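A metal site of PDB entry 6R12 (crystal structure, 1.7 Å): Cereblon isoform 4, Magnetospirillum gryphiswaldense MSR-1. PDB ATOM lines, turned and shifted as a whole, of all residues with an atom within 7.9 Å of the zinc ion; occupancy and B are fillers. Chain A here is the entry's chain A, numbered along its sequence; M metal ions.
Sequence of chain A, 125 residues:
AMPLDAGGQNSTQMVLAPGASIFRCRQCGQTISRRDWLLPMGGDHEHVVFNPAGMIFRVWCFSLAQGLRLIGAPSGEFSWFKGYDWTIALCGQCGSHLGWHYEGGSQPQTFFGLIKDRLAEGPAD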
ATOM      1  N   ARG A  24      -4.161  11.537  -7.861  1.00  0.00           N
ATOM      2  CA  ARG A  24      -4.001  10.203  -8.381  1.00  0.00           C
ATOM      3  C   ARG A  24      -5.200   9.324  -8.102  1.00  0.00           C
ATOM      4  O   ARG A  24      -5.992   9.705  -7.270  1.00  0.00           O
ATOM      5  CB  ARG A  24      -2.817   9.490  -7.703  1.00  0.00           C
ATOM      6  CG  ARG A  24      -1.496  10.162  -7.942  1.00  0.00           C
ATOM      7  CD  ARG A  24      -0.265   9.353  -7.357  1.00  0.00           C
ATOM      8  NE  ARG A  24       0.921  10.108  -7.783  1.00  0.00           N
ATOM      9  CZ  ARG A  24       1.472  10.048  -8.973  1.00  0.00           C
ATOM     10  NH1 ARG A  24       1.096   9.131  -9.858  1.00  0.00           N
ATOM     11  NH2 ARG A  24       2.475  10.882  -9.233  1.00  0.00           N
ATOM     12  N   CYS A  25      -5.407   8.245  -8.869  1.00  0.00           N
ATOM     13  CA  CYS A  25      -6.393   7.315  -8.550  1.00  0.00           C
ATOM     14  C   CYS A  25      -6.195   6.788  -7.104  1.00  0.00           C
ATOM     15  O   CYS A  25      -5.111   6.289  -6.822  1.00  0.00           O
ATOM     16  CB  CYS A  25      -6.428   6.178  -9.520  1.00  0.00           C
ATOM     17  SG  CYS A  25      -7.634   4.847  -9.202  1.00  0.00           S
ATOM     18  N   ARG A  26      -7.240   6.769  -6.295  1.00  0.00           N
ATOM     19  CA  ARG A  26      -7.139   6.285  -4.953  1.00  0.00           C
ATOM     20  C   ARG A  26      -6.895   4.798  -4.856  1.00  0.00           C
ATOM     21  O   ARG A  26      -6.300   4.367  -3.849  1.00  0.00           O
ATOM     22  CB  ARG A  26      -8.433   6.658  -4.219  1.00  0.00           C
ATOM     23  CG  ARG A  26      -8.595   6.084  -2.870  1.00  0.00           C
ATOM     24  CD  ARG A  26      -9.914   6.548  -2.379  1.00  0.00           C
ATOM     25  NE  ARG A  26     -10.086   5.917  -1.124  1.00  0.00           N
ATOM     26  CZ  ARG A  26     -11.070   6.108  -0.286  1.00  0.00           C
ATOM     27  NH1 ARG A  26     -12.055   6.996  -0.587  1.00  0.00           N
ATOM     28  NH2 ARG A  26     -11.114   5.335   0.826  1.00  0.00           N
ATOM     29  N   GLN A  27      -7.303   4.052  -5.862  1.00  0.00           N
ATOM     30  CA  GLN A  27      -7.126   2.601  -5.841  1.00  0.00           C
ATOM     31  C   GLN A  27      -5.761   2.094  -6.278  1.00  0.00           C
ATOM     32  O   GLN A  27      -5.330   1.073  -5.826  1.00  0.00           O
ATOM     33  CB  GLN A  27      -8.256   1.942  -6.616  1.00  0.00           C
ATOM     34  CG  GLN A  27      -9.602   2.408  -6.050  1.00  0.00           C
ATOM     35  CD  GLN A  27      -9.864   2.036  -4.667  1.00  0.00           C
ATOM     36  OE1 GLN A  27      -9.393   0.999  -4.203  1.00  0.00           O
ATOM     37  NE2 GLN A  27     -10.645   2.884  -3.951  1.00  0.00           N
ATOM     38  N   CYS A  28      -5.088   2.789  -7.145  1.00  0.00           N
ATOM     39  CA  CYS A  28      -3.879   2.311  -7.759  1.00  0.00           C
ATOM     40  C   CYS A  28      -2.775   3.253  -7.965  1.00  0.00           C
ATOM     41  O   CYS A  28      -1.672   2.878  -8.364  1.00  0.00           O
ATOM     42  CB  CYS A  28      -4.270   1.628  -9.054  1.00  0.00           C
ATOM     43  SG  CYS A  28      -4.560   2.854 -10.399  1.00  0.00           S
ATOM     44  N   GLY A  29      -3.017   4.568  -7.789  1.00  0.00           N
ATOM     45  CA  GLY A  29      -2.048   5.605  -7.936  1.00  0.00           C
ATOM     46  C   GLY A  29      -1.740   6.167  -9.287  1.00  0.00           C
ATOM     47  O   GLY A  29      -0.848   7.067  -9.450  1.00  0.00           O
ATOM     48  N   GLN A  30      -2.443   5.702 -10.307  1.00  0.00           N
ATOM     49  CA  GLN A  30      -2.307   6.352 -11.632  1.00  0.00           C
ATOM     50  C   GLN A  30      -2.469   7.854 -11.530  1.00  0.00           C
ATOM     51  O   GLN A  30      -3.363   8.328 -10.900  1.00  0.00           O
ATOM     52  CB  GLN A  30      -3.448   5.833 -12.562  1.00  0.00           C
ATOM     53  CG  GLN A  30      -3.601   6.466 -13.873  1.00  0.00           C
ATOM     54  CD  GLN A  30      -2.773   5.795 -14.933  1.00  0.00           C
ATOM     55  OE1 GLN A  30      -1.635   5.503 -14.754  1.00  0.00           O
ATOM     56  NE2 GLN A  30      -3.415   5.536 -16.085  1.00  0.00           N
ATOM     57  N   THR A  31      -1.579   8.597 -12.179  1.00  0.00           N
ATOM     58  CA  THR A  31      -1.663  10.044 -12.249  1.00  0.00           C
ATOM     59  C   THR A  31      -2.906  10.419 -13.033  1.00  0.00           C
ATOM     60  O   THR A  31      -3.116   9.942 -14.122  1.00  0.00           O
ATOM     61  CB  THR A  31      -0.407  10.599 -13.073  1.00  0.00           C
ATOM     62  OG1 THR A  31       0.804   9.939 -12.701  1.00  0.00           O
ATOM     63  CG2 THR A  31      -0.325  12.046 -12.851  1.00  0.00           C
ATOM     64  N   ILE A  32      -3.710  11.327 -12.495  1.00  0.00           N
ATOM     65  CA  ILE A  32      -4.959  11.714 -13.130  1.00  0.00           C
ATOM     66  C   ILE A  32      -5.073  13.209 -13.347  1.00  0.00           C
ATOM     67  O   ILE A  32      -5.404  13.584 -14.426  1.00  0.00           O
ATOM     68  CB  ILE A  32      -6.227  11.327 -12.259  1.00  0.00           C
ATOM     69  CG1 ILE A  32      -6.259   9.796 -12.025  1.00  0.00           C
ATOM     70  CG2 ILE A  32      -7.554  11.681 -13.046  1.00  0.00           C
ATOM     71  CD1 ILE A  32      -6.350   8.915 -13.238  1.00  0.00           C
ATOM     72  N   GLY A  67      -4.598   9.792 -17.810  1.00  0.00           N
ATOM     73  CA  GLY A  67      -4.556   8.426 -17.282  1.00  0.00           C
ATOM     74  C   GLY A  67      -5.900   7.755 -17.153  1.00  0.00           C
ATOM     75  O   GLY A  67      -6.072   6.761 -16.381  1.00  0.00           O
ATOM     76  N   LEU A  90     -13.087   5.978 -16.771  1.00  0.00           N
ATOM     77  CA  LEU A  90     -12.462   5.018 -15.853  1.00  0.00           C
ATOM     78  C   LEU A  90     -10.981   5.329 -15.704  1.00  0.00           C
ATOM     79  O   LEU A  90     -10.324   5.938 -16.587  1.00  0.00           O
ATOM     80  CB  LEU A  90     -12.574   3.614 -16.384  1.00  0.00           C
ATOM     81  CG  LEU A  90     -13.976   3.115 -16.678  1.00  0.00           C
ATOM     82  CD1 LEU A  90     -14.047   1.650 -17.130  1.00  0.00           C
ATOM     83  CD2 LEU A  90     -14.998   3.423 -15.563  1.00  0.00           C
ATOM     84  N   CYS A  91     -10.479   4.968 -14.537  1.00  0.00           N
ATOM     85  CA  CYS A  91      -9.012   4.876 -14.352  1.00  0.00           C
ATOM     86  C   CYS A  91      -8.476   3.972 -15.440  1.00  0.00           C
ATOM     87  O   CYS A  91      -8.901   2.852 -15.585  1.00  0.00           O
ATOM     88  CB  CYS A  91      -8.644   4.393 -12.977  1.00  0.00           C
ATOM     89  SG  CYS A  91      -6.781   4.249 -12.844  1.00  0.00           S
ATOM     90  N   GLY A  92      -7.527   4.497 -16.261  1.00  0.00           N
ATOM     91  CA  GLY A  92      -6.954   3.720 -17.324  1.00  0.00           C
ATOM     92  C   GLY A  92      -6.122   2.545 -16.847  1.00  0.00           C
ATOM     93  O   GLY A  92      -5.871   1.689 -17.618  1.00  0.00           O
ATOM     94  N   GLN A  93      -5.676   2.564 -15.614  1.00  0.00           N
ATOM     95  CA  GLN A  93      -4.771   1.607 -15.092  1.00  0.00           C
ATOM     96  C   GLN A  93      -5.644   0.492 -14.450  1.00  0.00           C
ATOM     97  O   GLN A  93      -5.563  -0.643 -14.878  1.00  0.00           O
ATOM     98  CB  GLN A  93      -3.791   2.208 -14.117  1.00  0.00           C
ATOM     99  CG  GLN A  93      -2.863   1.163 -13.508  1.00  0.00           C
ATOM    100  CD  GLN A  93      -1.630   1.885 -12.989  1.00  0.00           C
ATOM    101  OE1 GLN A  93      -0.625   1.950 -13.719  1.00  0.00           O
ATOM    102  NE2 GLN A  93      -1.733   2.476 -11.791  1.00  0.00           N
ATOM    103  N   CYS A  94      -6.517   0.860 -13.500  1.00  0.00           N
ATOM    104  CA  CYS A  94      -7.204  -0.120 -12.751  1.00  0.00           C
ATOM    105  C   CYS A  94      -8.714  -0.354 -13.050  1.00  0.00           C
ATOM    106  O   CYS A  94      -9.321  -1.275 -12.469  1.00  0.00           O
ATOM    107  CB  CYS A  94      -7.084   0.047 -11.243  1.00  0.00           C
ATOM    108  SG  CYS A  94      -8.079   1.405 -10.525  1.00  0.00           S
ATOM    109  N   GLY A  95      -9.280   0.559 -13.861  1.00  0.00           N
ATOM    110  CA  GLY A  95     -10.686   0.483 -14.215  1.00  0.00           C
ATOM    111  C   GLY A  95     -11.682   1.122 -13.212  1.00  0.00           C
ATOM    112  O   GLY A  95     -12.906   1.089 -13.440  1.00  0.00           O
ATOM    113  N   SER A  96     -11.229   1.664 -12.105  1.00  0.00           N
ATOM    114  CA  SER A  96     -12.059   2.415 -11.126  1.00  0.00           C
ATOM    115  C   SER A  96     -12.846   3.536 -11.797  1.00  0.00           C
ATOM    116  O   SER A  96     -12.297   4.227 -12.660  1.00  0.00           O
ATOM    117  CB  SER A  96     -11.241   2.950  -9.987  1.00  0.00           C
ATOM    118  OG  SER A  96     -11.952   3.769  -9.091  1.00  0.00           O
ATOM    119  N   HIS A  97     -14.167   3.645 -11.483  1.00  0.00           N
ATOM    120  CA  HIS A  97     -14.928   4.719 -12.087  1.00  0.00           C
ATOM    121  C   HIS A  97     -14.595   6.037 -11.405  1.00  0.00           C
ATOM    122  O   HIS A  97     -14.963   6.233 -10.263  1.00  0.00           O
ATOM    123  CB  HIS A  97     -16.430   4.409 -12.062  1.00  0.00           C
ATOM    124  CG  HIS A  97     -17.243   5.536 -12.588  1.00  0.00           C
ATOM    125  ND1 HIS A  97     -18.556   5.759 -12.173  1.00  0.00           N
ATOM    126  CD2 HIS A  97     -16.947   6.480 -13.510  1.00  0.00           C
ATOM    127  CE1 HIS A  97     -19.005   6.807 -12.846  1.00  0.00           C
ATOM    128  NE2 HIS A  97     -18.055   7.286 -13.617  1.00  0.00           N
ATOM    129  N   LEU A  98     -13.878   6.926 -12.096  1.00  0.00           N
ATOM    130  CA  LEU A  98     -13.409   8.186 -11.562  1.00  0.00           C
ATOM    131  C   LEU A  98     -14.237   9.361 -11.831  1.00  0.00           C
ATOM    132  O   LEU A  98     -14.143  10.375 -11.114  1.00  0.00           O
ATOM    133  CB  LEU A  98     -11.946   8.439 -11.907  1.00  0.00           C
ATOM    134  CG  LEU A  98     -10.911   7.371 -11.385  1.00  0.00           C
ATOM    135  CD1 LEU A  98      -9.499   7.799 -11.735  1.00  0.00           C
ATOM    136  CD2 LEU A  98     -11.074   7.170  -9.889  1.00  0.00           C
ATOM    137  N   ARG A 118     -12.768   9.629  -4.909  1.00  0.00           N
ATOM    138  CA  ARG A 118     -12.161   8.557  -5.592  1.00  0.00           C
ATOM    139  C   ARG A 118     -10.709   8.890  -6.023  1.00  0.00           C
ATOM    140  O   ARG A 118     -10.088   8.062  -6.661  1.00  0.00           O
ATOM    141  CB  ARG A 118     -13.042   8.152  -6.774  1.00  0.00           C
ATOM    142  CG  ARG A 118     -14.374   7.624  -6.245  1.00  0.00           C
ATOM    143  CD  ARG A 118     -15.182   6.849  -7.251  1.00  0.00           C
ATOM    144  NE  ARG A 118     -16.534   6.611  -6.766  1.00  0.00           N
ATOM    145  CZ  ARG A 118     -17.503   5.989  -7.438  1.00  0.00           C
ATOM    146  NH1 ARG A 118     -17.311   5.634  -8.720  1.00  0.00           N
ATOM    147  NH2 ARG A 118     -18.772   5.847  -6.910  1.00  0.00           N
HETATM  148 ZN    ZN M   1      -6.814   3.285 -10.653  1.00  0.00          ZN
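SG of Cys 25 sits close to N of Gln 27 (3.4 Å). The backbone NH (N) of Cys 25 lies within hydrogen-bond range of the backbone carbonyl oxygen (O) of Gln 30 (2.9 Å). The backbone carbonyl oxygen (O) of Cys 28 lies within hydrogen-bond range of the side-chain amide nitrogen (NE2) of Gln 93, at 3.5 Å. O of Ser 96 is in hydrogen-bond range of N of Cys 91, at 2.7 Å. N of Gln 30 lies close to SG of Cys 28. SG of Cys 94 sits close to N of Ser 96 (3.5 Å). SG of Cys 91 sits close to N of Gln 93 (3.4 Å).
The nearest printed residue that does not touch the zinc ion is Ser 96 (4.5 Å).
The zinc ion is bound by SG of Cys 94 (2.3 Å), SG of Cys 25 (2.3 Å), SG of Cys 28 (2.3 Å) and SG of Cys 91 (2.4 Å).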
